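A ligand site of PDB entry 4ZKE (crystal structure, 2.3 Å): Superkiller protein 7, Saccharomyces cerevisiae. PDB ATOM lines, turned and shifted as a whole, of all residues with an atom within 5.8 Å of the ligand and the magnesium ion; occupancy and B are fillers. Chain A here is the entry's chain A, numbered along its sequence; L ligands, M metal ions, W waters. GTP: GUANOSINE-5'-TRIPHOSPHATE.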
ATOM      1  N   GLY A  26      19.693  -9.638 -15.216  1.00  0.00           N
ATOM      2  CA  GLY A  26      18.359 -10.223 -15.191  1.00  0.00           C
ATOM      3  C   GLY A  26      18.292 -11.567 -15.888  1.00  0.00           C
ATOM      4  O   GLY A  26      19.215 -11.951 -16.611  1.00  0.00           O
ATOM      5  N   ASP A  27      17.187 -12.278 -15.661  1.00  0.00           N
ATOM      6  CA  ASP A  27      16.962 -13.576 -16.295  1.00  0.00           C
ATOM      7  C   ASP A  27      16.891 -13.441 -17.807  1.00  0.00           C
ATOM      8  O   ASP A  27      16.783 -12.337 -18.340  1.00  0.00           O
ATOM      9  CB  ASP A  27      15.658 -14.200 -15.788  1.00  0.00           C
ATOM     10  CG  ASP A  27      15.647 -14.384 -14.294  1.00  0.00           C
ATOM     11  OD1 ASP A  27      16.734 -14.377 -13.676  1.00  0.00           O
ATOM     12  OD2 ASP A  27      14.541 -14.548 -13.730  1.00  0.00           O
ATOM     13  N   THR A  28      16.948 -14.583 -18.498  1.00  0.00           N
ATOM     14  CA  THR A  28      16.751 -14.595 -19.939  1.00  0.00           C
ATOM     15  C   THR A  28      15.338 -14.116 -20.246  1.00  0.00           C
ATOM     16  O   THR A  28      14.434 -14.268 -19.419  1.00  0.00           O
ATOM     17  CB  THR A  28      16.979 -16.001 -20.544  1.00  0.00           C
ATOM     18  OG1 THR A  28      16.951 -15.920 -21.973  1.00  0.00           O
ATOM     19  CG2 THR A  28      15.902 -16.977 -20.077  1.00  0.00           C
ATOM     20  N   ASN A  29      15.162 -13.511 -21.424  1.00  0.00           N
ATOM     21  CA  ASN A  29      13.858 -13.044 -21.886  1.00  0.00           C
ATOM     22  C   ASN A  29      13.338 -11.833 -21.096  1.00  0.00           C
ATOM     23  O   ASN A  29      12.195 -11.443 -21.250  1.00  0.00           O
ATOM     24  CB  ASN A  29      12.847 -14.195 -21.808  1.00  0.00           C
ATOM     25  CG  ASN A  29      11.656 -13.977 -22.714  1.00  0.00           C
ATOM     26  OD1 ASN A  29      11.804 -13.896 -23.936  1.00  0.00           O
ATOM     27  ND2 ASN A  29      10.467 -13.909 -22.131  1.00  0.00           N
ATOM     28  N   ALA A  30      14.200 -11.243 -20.270  1.00  0.00           N
ATOM     29  CA  ALA A  30      13.793 -10.094 -19.454  1.00  0.00           C
ATOM     30  C   ALA A  30      13.616  -8.836 -20.311  1.00  0.00           C
ATOM     31  O   ALA A  30      12.773  -7.988 -20.003  1.00  0.00           O
ATOM     32  CB  ALA A  30      14.820  -9.848 -18.362  1.00  0.00           C
ATOM     33  N   GLY A  31      14.409  -8.719 -21.375  1.00  0.00           N
ATOM     34  CA  GLY A  31      14.333  -7.591 -22.282  1.00  0.00           C
ATOM     35  C   GLY A  31      15.522  -6.664 -22.171  1.00  0.00           C
ATOM     36  O   GLY A  31      15.459  -5.507 -22.587  1.00  0.00           O
ATOM     37  N   LYS A  32      16.623  -7.166 -21.628  1.00  0.00           N
ATOM     38  CA  LYS A  32      17.831  -6.367 -21.434  1.00  0.00           C
ATOM     39  C   LYS A  32      18.401  -5.855 -22.748  1.00  0.00           C
ATOM     40  O   LYS A  32      18.642  -4.659 -22.914  1.00  0.00           O
ATOM     41  CB  LYS A  32      18.887  -7.179 -20.685  1.00  0.00           C
ATOM     42  CG  LYS A  32      18.426  -7.683 -19.337  1.00  0.00           C
ATOM     43  CD  LYS A  32      19.529  -8.395 -18.589  1.00  0.00           C
ATOM     44  CE  LYS A  32      19.928  -9.706 -19.240  1.00  0.00           C
ATOM     45  NZ  LYS A  32      18.820 -10.698 -19.236  1.00  0.00           N
ATOM     46  N   SER A  33      18.617  -6.765 -23.695  1.00  0.00           N
ATOM     47  CA  SER A  33      19.198  -6.401 -24.987  1.00  0.00           C
ATOM     48  C   SER A  33      18.261  -5.464 -25.758  1.00  0.00           C
ATOM     49  O   SER A  33      18.705  -4.456 -26.305  1.00  0.00           O
ATOM     50  CB  SER A  33      19.503  -7.645 -25.811  1.00  0.00           C
ATOM     51  OG  SER A  33      20.496  -8.442 -25.169  1.00  0.00           O
ATOM     52  N   THR A  34      16.984  -5.808 -25.806  1.00  0.00           N
ATOM     53  CA  THR A  34      15.982  -4.969 -26.453  1.00  0.00           C
ATOM     54  C   THR A  34      15.996  -3.554 -25.878  1.00  0.00           C
ATOM     55  O   THR A  34      16.170  -2.583 -26.616  1.00  0.00           O
ATOM     56  CB  THR A  34      14.569  -5.573 -26.300  1.00  0.00           C
ATOM     57  OG1 THR A  34      14.524  -6.854 -26.939  1.00  0.00           O
ATOM     58  CG2 THR A  34      13.512  -4.662 -26.935  1.00  0.00           C
ATOM     59  N   LEU A  35      15.813  -3.464 -24.565  1.00  0.00           N
ATOM     60  CA  LEU A  35      15.722  -2.167 -23.896  1.00  0.00           C
ATOM     61  C   LEU A  35      16.961  -1.338 -24.149  1.00  0.00           C
ATOM     62  O   LEU A  35      16.891  -0.142 -24.422  1.00  0.00           O
ATOM     63  CB  LEU A  35      15.516  -2.369 -22.394  1.00  0.00           C
ATOM     64  CG  LEU A  35      15.337  -1.088 -21.566  1.00  0.00           C
ATOM     65  CD1 LEU A  35      14.329  -1.337 -20.456  1.00  0.00           C
ATOM     66  CD2 LEU A  35      16.665  -0.628 -20.976  1.00  0.00           C
ATOM     67  N   SER A  64       9.738 -14.918 -33.092  1.00  0.00           N
ATOM     68  CA  SER A  64       9.327 -15.143 -31.713  1.00  0.00           C
ATOM     69  C   SER A  64      10.361 -14.584 -30.728  1.00  0.00           C
ATOM     70  O   SER A  64      10.034 -14.271 -29.582  1.00  0.00           O
ATOM     71  CB  SER A  64       9.139 -16.640 -31.460  1.00  0.00           C
ATOM     72  OG  SER A  64       8.342 -17.234 -32.466  1.00  0.00           O
ATOM     73  N   SER A  65      11.609 -14.465 -31.180  1.00  0.00           N
ATOM     74  CA  SER A  65      12.709 -14.055 -30.321  1.00  0.00           C
ATOM     75  C   SER A  65      13.306 -12.707 -30.718  1.00  0.00           C
ATOM     76  O   SER A  65      13.872 -12.007 -29.872  1.00  0.00           O
ATOM     77  CB  SER A  65      13.814 -15.114 -30.347  1.00  0.00           C
ATOM     78  OG  SER A  65      13.375 -16.331 -29.788  1.00  0.00           O
ATOM     79  N   SER A  66      13.186 -12.343 -31.983  1.00  0.00           N
ATOM     80  CA  SER A  66      13.931 -11.212 -32.524  1.00  0.00           C
ATOM     81  C   SER A  66      13.117  -9.922 -32.660  1.00  0.00           C
ATOM     82  O   SER A  66      11.907  -9.951 -32.875  1.00  0.00           O
ATOM     83  CB  SER A  66      14.505 -11.575 -33.896  1.00  0.00           C
ATOM     84  OG  SER A  66      15.326 -10.532 -34.405  1.00  0.00           O
ATOM     85  N   ASN A  67      13.818  -8.799 -32.525  1.00  0.00           N
ATOM     86  CA  ASN A  67      13.299  -7.486 -32.909  1.00  0.00           C
ATOM     87  C   ASN A  67      14.479  -6.618 -33.333  1.00  0.00           C
ATOM     88  O   ASN A  67      15.628  -7.033 -33.207  1.00  0.00           O
ATOM     89  CB  ASN A  67      12.520  -6.834 -31.758  1.00  0.00           C
ATOM     90  CG  ASN A  67      13.401  -6.462 -30.585  1.00  0.00           C
ATOM     91  OD1 ASN A  67      14.085  -5.430 -30.610  1.00  0.00           O
ATOM     92  ND2 ASN A  67      13.390  -7.281 -29.541  1.00  0.00           N
ATOM     93  N   LYS A  70      17.230  -5.417 -30.267  1.00  0.00           N
ATOM     94  CA  LYS A  70      18.110  -6.377 -29.612  1.00  0.00           C
ATOM     95  C   LYS A  70      19.220  -6.856 -30.540  1.00  0.00           C
ATOM     96  O   LYS A  70      20.297  -7.241 -30.073  1.00  0.00           O
ATOM     97  CB  LYS A  70      17.308  -7.568 -29.076  1.00  0.00           C
ATOM     98  CG  LYS A  70      16.581  -8.357 -30.135  1.00  0.00           C
ATOM     99  CD  LYS A  70      15.943  -9.610 -29.540  1.00  0.00           C
ATOM    100  CE  LYS A  70      16.971 -10.686 -29.254  1.00  0.00           C
ATOM    101  NZ  LYS A  70      16.352 -11.947 -28.747  1.00  0.00           N
ATOM    102  N   ASP A  74      22.828  -8.117 -29.837  1.00  0.00           N
ATOM    103  CA  ASP A  74      23.044  -9.475 -30.289  1.00  0.00           C
ATOM    104  C   ASP A  74      23.547  -9.412 -31.720  1.00  0.00           C
ATOM    105  O   ASP A  74      22.820  -9.719 -32.669  1.00  0.00           O
ATOM    106  CB  ASP A  74      21.766 -10.308 -30.182  1.00  0.00           C
ATOM    107  CG  ASP A  74      21.422 -10.678 -28.758  1.00  0.00           C
ATOM    108  OD1 ASP A  74      22.119 -10.203 -27.838  1.00  0.00           O
ATOM    109  OD2 ASP A  74      20.447 -11.438 -28.551  1.00  0.00           O
ATOM    110  N   GLY A  83      19.053 -16.707 -30.860  1.00  0.00           N
ATOM    111  CA  GLY A  83      17.952 -15.847 -30.442  1.00  0.00           C
ATOM    112  C   GLY A  83      18.062 -15.339 -29.013  1.00  0.00           C
ATOM    113  O   GLY A  83      17.068 -14.925 -28.423  1.00  0.00           O
ATOM    114  N   PHE A  84      19.273 -15.362 -28.461  1.00  0.00           N
ATOM    115  CA  PHE A  84      19.524 -14.813 -27.127  1.00  0.00           C
ATOM    116  C   PHE A  84      21.004 -14.483 -26.933  1.00  0.00           C
ATOM    117  O   PHE A  84      21.861 -14.989 -27.662  1.00  0.00           O
ATOM    118  CB  PHE A  84      19.057 -15.796 -26.051  1.00  0.00           C
ATOM    119  CG  PHE A  84      19.696 -17.154 -26.142  1.00  0.00           C
ATOM    120  CD1 PHE A  84      20.909 -17.396 -25.535  1.00  0.00           C
ATOM    121  CD2 PHE A  84      19.055 -18.193 -26.810  1.00  0.00           C
ATOM    122  CE1 PHE A  84      21.502 -18.650 -25.610  1.00  0.00           C
ATOM    123  CE2 PHE A  84      19.639 -19.437 -26.889  1.00  0.00           C
ATOM    124  CZ  PHE A  84      20.855 -19.667 -26.287  1.00  0.00           C
ATOM    125  N   SER A  85      21.290 -13.634 -25.959  1.00  0.00           N
ATOM    126  CA  SER A  85      22.651 -13.174 -25.726  1.00  0.00           C
ATOM    127  C   SER A  85      23.517 -14.280 -25.124  1.00  0.00           C
ATOM    128  O   SER A  85      23.046 -15.089 -24.326  1.00  0.00           O
ATOM    129  CB  SER A  85      22.658 -11.950 -24.799  1.00  0.00           C
ATOM    130  OG  SER A  85      21.843 -10.915 -25.331  1.00  0.00           O
ATOM    131  N   MET A  86      24.788 -14.295 -25.518  1.00  0.00           N
ATOM    132  CA  MET A  86      25.753 -15.287 -25.038  1.00  0.00           C
ATOM    133  C   MET A  86      27.014 -14.602 -24.531  1.00  0.00           C
ATOM    134  O   MET A  86      27.714 -15.148 -23.666  1.00  0.00           O
ATOM    135  CB  MET A  86      26.105 -16.263 -26.164  1.00  0.00           C
ATOM    136  CG  MET A  86      24.932 -17.068 -26.679  1.00  0.00           C
ATOM    137  SD  MET A  86      25.245 -17.808 -28.292  1.00  0.00           S
ATOM    138  CE  MET A  86      26.608 -18.887 -27.920  1.00  0.00           C
ATOM    139  N   ASP A 108      25.781  -4.964 -21.302  1.00  0.00           N
ATOM    140  CA  ASP A 108      24.782  -6.010 -21.453  1.00  0.00           C
ATOM    141  C   ASP A 108      25.366  -7.333 -20.983  1.00  0.00           C
ATOM    142  O   ASP A 108      26.561  -7.576 -21.141  1.00  0.00           O
ATOM    143  CB  ASP A 108      24.326  -6.116 -22.913  1.00  0.00           C
ATOM    144  CG  ASP A 108      23.104  -7.014 -23.085  1.00  0.00           C
ATOM    145  OD1 ASP A 108      22.394  -7.268 -22.095  1.00  0.00           O
ATOM    146  OD2 ASP A 108      22.857  -7.448 -24.235  1.00  0.00           O
ATOM    147  N   THR A 109      24.536  -8.180 -20.384  1.00  0.00           N
ATOM    148  CA  THR A 109      24.983  -9.489 -19.922  1.00  0.00           C
ATOM    149  C   THR A 109      23.946 -10.543 -20.257  1.00  0.00           C
ATOM    150  O   THR A 109      22.757 -10.248 -20.335  1.00  0.00           O
ATOM    151  CB  THR A 109      25.247  -9.497 -18.398  1.00  0.00           C
ATOM    152  OG1 THR A 109      24.014  -9.360 -17.687  1.00  0.00           O
ATOM    153  CG2 THR A 109      26.198  -8.386 -18.001  1.00  0.00           C
ATOM    154  N   PRO A 110      24.399 -11.787 -20.466  1.00  0.00           N
ATOM    155  CA  PRO A 110      23.455 -12.859 -20.797  1.00  0.00           C
ATOM    156  C   PRO A 110      22.671 -13.319 -19.576  1.00  0.00           C
ATOM    157  O   PRO A 110      23.222 -13.349 -18.475  1.00  0.00           O
ATOM    158  CB  PRO A 110      24.356 -13.970 -21.330  1.00  0.00           C
ATOM    159  CG  PRO A 110      25.656 -13.754 -20.638  1.00  0.00           C
ATOM    160  CD  PRO A 110      25.792 -12.272 -20.429  1.00  0.00           C
ATOM    161  N   GLY A 111      21.408 -13.679 -19.778  1.00  0.00           N
ATOM    162  CA  GLY A 111      20.544 -14.157 -18.710  1.00  0.00           C
ATOM    163  C   GLY A 111      20.386 -15.675 -18.676  1.00  0.00           C
ATOM    164  O   GLY A 111      20.171 -16.248 -17.610  1.00  0.00           O
ATOM    165  N   SER A 112      20.455 -16.319 -19.841  1.00  0.00           N
ATOM    166  CA  SER A 112      20.360 -17.775 -19.908  1.00  0.00           C
ATOM    167  C   SER A 112      21.434 -18.393 -19.038  1.00  0.00           C
ATOM    168  O   SER A 112      22.618 -18.083 -19.181  1.00  0.00           O
ATOM    169  CB  SER A 112      20.472 -18.270 -21.352  1.00  0.00           C
ATOM    170  OG  SER A 112      21.712 -17.888 -21.924  1.00  0.00           O
ATOM    171  N   ASN A 179       9.912  -4.118 -16.475  1.00  0.00           N
ATOM    172  CA  ASN A 179       9.851  -4.088 -17.927  1.00  0.00           C
ATOM    173  C   ASN A 179       8.641  -4.821 -18.515  1.00  0.00           C
ATOM    174  O   ASN A 179       7.934  -5.539 -17.812  1.00  0.00           O
ATOM    175  CB  ASN A 179      11.142  -4.691 -18.501  1.00  0.00           C
ATOM    176  CG  ASN A 179      11.396  -4.297 -19.950  1.00  0.00           C
ATOM    177  OD1 ASN A 179      10.894  -3.279 -20.438  1.00  0.00           O
ATOM    178  ND2 ASN A 179      12.164  -5.121 -20.649  1.00  0.00           N
ATOM    179  N   LYS A 180       8.416  -4.608 -19.819  1.00  0.00           N
ATOM    180  CA  LYS A 180       7.307  -5.223 -20.551  1.00  0.00           C
ATOM    181  C   LYS A 180       5.968  -4.807 -19.955  1.00  0.00           C
ATOM    182  O   LYS A 180       5.020  -5.598 -19.923  1.00  0.00           O
ATOM    183  CB  LYS A 180       7.430  -6.745 -20.551  1.00  0.00           C
ATOM    184  CG  LYS A 180       8.766  -7.266 -21.047  1.00  0.00           C
ATOM    185  CD  LYS A 180       8.638  -8.665 -21.628  1.00  0.00           C
ATOM    186  CE  LYS A 180       9.991  -9.306 -21.847  1.00  0.00           C
ATOM    187  NZ  LYS A 180       9.856 -10.709 -22.323  1.00  0.00           N
ATOM    188  N   ALA A 181       5.890  -3.569 -19.479  1.00  0.00           N
ATOM    189  CA  ALA A 181       4.667  -3.041 -18.898  1.00  0.00           C
ATOM    190  C   ALA A 181       3.546  -3.001 -19.936  1.00  0.00           C
ATOM    191  O   ALA A 181       2.359  -3.007 -19.582  1.00  0.00           O
ATOM    192  CB  ALA A 181       4.906  -1.655 -18.325  1.00  0.00           C
ATOM    193  N   ASP A 182       3.907  -2.981 -21.215  1.00  0.00           N
ATOM    194  CA  ASP A 182       2.921  -2.964 -22.298  1.00  0.00           C
ATOM    195  C   ASP A 182       2.144  -4.277 -22.368  1.00  0.00           C
ATOM    196  O   ASP A 182       0.958  -4.274 -22.715  1.00  0.00           O
ATOM    197  CB  ASP A 182       3.612  -2.699 -23.636  1.00  0.00           C
ATOM    198  CG  ASP A 182       4.654  -3.749 -23.978  1.00  0.00           C
ATOM    199  OD1 ASP A 182       5.581  -3.944 -23.157  1.00  0.00           O
ATOM    200  OD2 ASP A 182       4.556  -4.376 -25.046  1.00  0.00           O
ATOM    201  N   LEU A 183       2.793  -5.388 -22.024  1.00  0.00           N
ATOM    202  CA  LEU A 183       2.150  -6.695 -22.081  1.00  0.00           C
ATOM    203  C   LEU A 183       1.133  -6.886 -20.960  1.00  0.00           C
ATOM    204  O   LEU A 183       0.455  -7.913 -20.905  1.00  0.00           O
ATOM    205  CB  LEU A 183       3.187  -7.803 -22.018  1.00  0.00           C
ATOM    206  CG  LEU A 183       4.096  -7.985 -23.249  1.00  0.00           C
ATOM    207  CD1 LEU A 183       5.083  -9.112 -22.992  1.00  0.00           C
ATOM    208  CD2 LEU A 183       3.289  -8.257 -24.504  1.00  0.00           C
ATOM    209  N   CYS A 218       8.603   0.403 -17.293  1.00  0.00           N
ATOM    210  CA  CYS A 218       8.958   0.751 -18.657  1.00  0.00           C
ATOM    211  C   CYS A 218       8.612  -0.351 -19.648  1.00  0.00           C
ATOM    212  O   CYS A 218       8.231  -1.457 -19.275  1.00  0.00           O
ATOM    213  CB  CYS A 218      10.444   1.064 -18.756  1.00  0.00           C
ATOM    214  SG  CYS A 218      11.504  -0.338 -18.331  1.00  0.00           S
ATOM    215  N   SER A 219       8.773  -0.007 -20.927  1.00  0.00           N
ATOM    216  CA  SER A 219       8.721  -0.976 -22.011  1.00  0.00           C
ATOM    217  C   SER A 219       9.919  -0.741 -22.933  1.00  0.00           C
ATOM    218  O   SER A 219       9.977   0.268 -23.635  1.00  0.00           O
ATOM    219  CB  SER A 219       7.416  -0.859 -22.811  1.00  0.00           C
ATOM    220  OG  SER A 219       7.384  -1.789 -23.870  1.00  0.00           O
ATOM    221  N   GLY A 220      10.878  -1.658 -22.897  1.00  0.00           N
ATOM    222  CA  GLY A 220      12.085  -1.503 -23.680  1.00  0.00           C
ATOM    223  C   GLY A 220      11.802  -1.630 -25.173  1.00  0.00           C
ATOM    224  O   GLY A 220      12.501  -1.042 -25.994  1.00  0.00           O
ATOM    225  N   LEU A 221      10.780  -2.411 -25.513  1.00  0.00           N
ATOM    226  CA  LEU A 221      10.413  -2.611 -26.909  1.00  0.00           C
ATOM    227  C   LEU A 221       9.755  -1.368 -27.486  1.00  0.00           C
ATOM    228  O   LEU A 221      10.157  -0.883 -28.548  1.00  0.00           O
ATOM    229  CB  LEU A 221       9.476  -3.808 -27.044  1.00  0.00           C
ATOM    230  CG  LEU A 221       9.010  -4.155 -28.450  1.00  0.00           C
ATOM    231  CD1 LEU A 221      10.186  -4.348 -29.408  1.00  0.00           C
ATOM    232  CD2 LEU A 221       8.157  -5.408 -28.415  1.00  0.00           C
ATOM    233  N   LEU A 222       8.755  -0.844 -26.792  1.00  0.00           N
ATOM    234  CA  LEU A 222       8.032   0.342 -27.245  1.00  0.00           C
ATOM    235  C   LEU A 222       8.744   1.635 -26.844  1.00  0.00           C
ATOM    236  O   LEU A 222       8.450   2.704 -27.381  1.00  0.00           O
ATOM    237  CB  LEU A 222       6.616   0.350 -26.675  1.00  0.00           C
ATOM    238  CG  LEU A 222       5.756  -0.879 -26.990  1.00  0.00           C
ATOM    239  CD1 LEU A 222       4.371  -0.728 -26.394  1.00  0.00           C
ATOM    240  CD2 LEU A 222       5.679  -1.130 -28.490  1.00  0.00           C
HETATM  241  PG  GTP L   1      18.799 -12.746 -22.687  1.00  0.00           P
HETATM  242  O1G GTP L   1      19.822 -12.148 -23.632  1.00  0.00           O
HETATM  243  O2G GTP L   1      18.668 -14.215 -22.998  1.00  0.00           O
HETATM  244  O3G GTP L   1      19.232 -12.577 -21.246  1.00  0.00           O
HETATM  245  O3B GTP L   1      17.374 -12.037 -22.919  1.00  0.00           O
HETATM  246  PB  GTP L   1      17.198 -10.456 -22.702  1.00  0.00           P
HETATM  247  O1B GTP L   1      18.357  -9.737 -23.355  1.00  0.00           O
HETATM  248  O2B GTP L   1      17.118 -10.107 -21.234  1.00  0.00           O
HETATM  249  O3A GTP L   1      15.814 -10.066 -23.432  1.00  0.00           O
HETATM  250  PA  GTP L   1      15.630  -9.897 -25.029  1.00  0.00           P
HETATM  251  O1A GTP L   1      16.048  -8.502 -25.424  1.00  0.00           O
HETATM  252  O2A GTP L   1      16.375 -10.942 -25.821  1.00  0.00           O
HETATM  253  O5' GTP L   1      14.040 -10.053 -25.238  1.00  0.00           O
HETATM  254  C5' GTP L   1      13.366 -11.268 -24.982  1.00  0.00           C
HETATM  255  C4' GTP L   1      12.042 -11.244 -25.750  1.00  0.00           C
HETATM  256  O4' GTP L   1      11.184 -10.325 -25.115  1.00  0.00           O
HETATM  257  C3' GTP L   1      12.214 -10.782 -27.182  1.00  0.00           C
HETATM  258  O3' GTP L   1      11.482 -11.636 -28.044  1.00  0.00           O
HETATM  259  C2' GTP L   1      11.628  -9.396 -27.232  1.00  0.00           C
HETATM  260  O2' GTP L   1      10.948  -9.163 -28.448  1.00  0.00           O
HETATM  261  C1' GTP L   1      10.690  -9.367 -26.030  1.00  0.00           C
HETATM  262  N9  GTP L   1      10.674  -8.047 -25.369  1.00  0.00           N
HETATM  263  C8  GTP L   1      11.738  -7.361 -24.849  1.00  0.00           C
HETATM  264  N7  GTP L   1      11.266  -6.199 -24.325  1.00  0.00           N
HETATM  265  C5  GTP L   1       9.934  -6.152 -24.494  1.00  0.00           C
HETATM  266  C6  GTP L   1       8.963  -5.205 -24.152  1.00  0.00           C
HETATM  267  O6  GTP L   1       9.268  -4.164 -23.570  1.00  0.00           O
HETATM  268  N1  GTP L   1       7.645  -5.453 -24.476  1.00  0.00           N
HETATM  269  C2  GTP L   1       7.290  -6.621 -25.127  1.00  0.00           C
HETATM  270  N2  GTP L   1       6.023  -6.854 -25.439  1.00  0.00           N
HETATM  271  N3  GTP L   1       8.251  -7.541 -25.455  1.00  0.00           N
HETATM  272  C4  GTP L   1       9.546  -7.312 -25.152  1.00  0.00           C
HETATM  273 MG    MG M   1      20.169 -10.279 -24.255  1.00  0.00          MG
HETATM  274  O   HOH W   1      21.162 -15.236 -22.684  1.00  0.00           O
HETATM  275  O   HOH W   2      12.804  -4.535 -23.248  1.00  0.00           O
HETATM  276  O   HOH W   3       8.009  -9.628 -28.533  1.00  0.00           O
HETATM  277  O   HOH W   4      21.262  -9.570 -22.591  1.00  0.00           O
HETATM  278  O   HOH W   5      19.147 -10.702 -26.092  1.00  0.00           O
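The backbone NH (N) of Ser 33 lies close to an oxygen (O1B) of the ligand. An oxygen (O1G) of the ligand sits close to the backbone NH (N) of Ser 85 (3.1 Å). The side-chain hydroxyl (OG1) of Thr 28 sits at hydrogen-bond distance from an oxygen (O2G) of the ligand (2.6 Å). N of Lys 32 is in hydrogen-bond range of O2B of the ligand (3.0 Å). NZ of Lys 32 is in salt-bridge range of O2B of the ligand, 2.7 Å away. The backbone NH of Thr 34 sits at hydrogen-bond distance from an oxygen (O1A) of the ligand, 2.9 Å away. O1A of the ligand lies within hydrogen-bond range of OG1 of Thr 34 (2.7 Å). The backbone NH (N) of Gly 31 lies within hydrogen-bond range of an oxygen (O3A) of the ligand (2.8 Å). N of Gly 111 sits at hydrogen-bond distance from O3G of the ligand (2.8 Å). A nitrogen (N1) of the ligand sits at hydrogen-bond distance from the side-chain carboxylate (OD1) of Asp 182, 2.9 Å away. The backbone NH (N) of Leu 221 sits at hydrogen-bond distance from an oxygen (O6) of the ligand (3.0 Å). An oxygen (O3') of the ligand lies within hydrogen-bond range of the backbone carbonyl oxygen (O) of Ser 65 (3.0 Å). The side-chain hydroxyl of Ser 219 sits at hydrogen-bond distance from an oxygen (O6) of the ligand (3.0 Å). O3B of the ligand lies within hydrogen-bond range of N of Asn 29, at 3.0 Å. The backbone NH (N) of Gly 220 lies within hydrogen-bond range of an oxygen (O6) of the ligand (3.1 Å). NZ of Lys 70 lies within salt-bridge range of O2A of the ligand (3.1 Å). An oxygen (O4') of the ligand sits at hydrogen-bond distance from the side-chain amino group (NZ) of Lys 180 (3.1 Å). ND2 of Asn 67 is in hydrogen-bond range of O2' of the ligand. N of Ala 30 sits at hydrogen-bond distance from O2B of the ligand, at 3.3 Å. O of Ser 64 lies within hydrogen-bond range of O3' of the ligand, 3.4 Å away.
OD2 of Asp 108 touches the magnesium ion (3.9 Å). Three residues have an atom within 4 Å of the magnesium ion: Ser 33, Ser 85 and Asp 108. Along chain A the residues within 4 Å of the magnesium ion span positions 33 to 108. The nearest printed residue that does not touch the magnesium ion is Asp 74 (4.1 Å).
Water W4 bridges the side-chain carboxylate (OD1) of Asp 108 (2.6 Å) and the backbone carbonyl oxygen (O) of Thr 109 (2.8 Å). Water W5 lies within hydrogen-bond range of an oxygen (O2A) of the ligand (2.8 Å) and the side-chain carboxylate of Asp 74 (2.9 Å). Water W1 lies within hydrogen-bond range of O of Ser 85 (2.5 Å), O2G of the ligand (2.7 Å), OG of Ser 112 (2.8 Å) and N of Gly 111 (3.3 Å).
The side-chain amino group (NZ) of Lys 32 sits at hydrogen-bond distance from the backbone carbonyl oxygen (O) of Asp 27 (2.8 Å). OG1 of Thr 34 lies within hydrogen-bond range of ND2 of Asn 67 (2.9 Å). The side-chain amino group of Lys 70 is in hydrogen-bond range of the backbone carbonyl oxygen of Ser 65 (2.7 Å). N of Leu 222 is in hydrogen-bond range of OG of Ser 219 (3.4 Å). The backbone NH (N) of Gly 220 is in hydrogen-bond range of the side-chain amide oxygen (OD1) of Asn 179 (2.9 Å). The backbone NH (N) of Lys 180 is in hydrogen-bond range of the backbone carbonyl oxygen (O) of Cys 218, 3.2 Å away. The backbone carbonyl oxygen of Ala 30 is in hydrogen-bond range of the side-chain amide nitrogen of Asn 179 (3.0 Å). OD1 of Asn 179 sits close to O of Cys 218, 3.4 Å away.
Asp 27 touches the ligand. Phe 84 touches the ligand. Pro 110 touches the ligand (C to O3G, 3.9 Å). Asn 179 touches the ligand (OD1 to O6, 3.6 Å). Leu 183 touches the ligand (CG to N2, 3.1 Å). Hydrophobic or aromatic side chains within 4 Å of the ligand: Ala 30, Phe 84, Leu 183 and Leu 221. 23 residues have an atom within 4 Å of the ligand: Asp 27, Thr 28, Asn 29, Ala 30, Gly 31, Lys 32, Ser 33, Thr 34, Ser 64, Ser 65, Asn 67, Lys 70, Phe 84, Ser 85, Pro 110, Gly 111, Asn 179, Lys 180, Asp 182, Leu 183, Ser 219, Gly 220 and Leu 221. The nearest printed residue that does not touch the ligand is Ser 112 (4.2 Å).
An oxygen (O1G) of the ligand binds the magnesium ion (2.0 Å). OG of Ser 33 binds the magnesium ion (2.1 Å). OG of Ser 85 is bound to the magnesium ion, 2.1 Å away. An oxygen (O1B) of the ligand is bound to the magnesium ion, at 2.1 Å. Water W4 is bound to the magnesium ion, at 2.1 Å. Water W5 is bound to the magnesium ion (2.1 Å).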
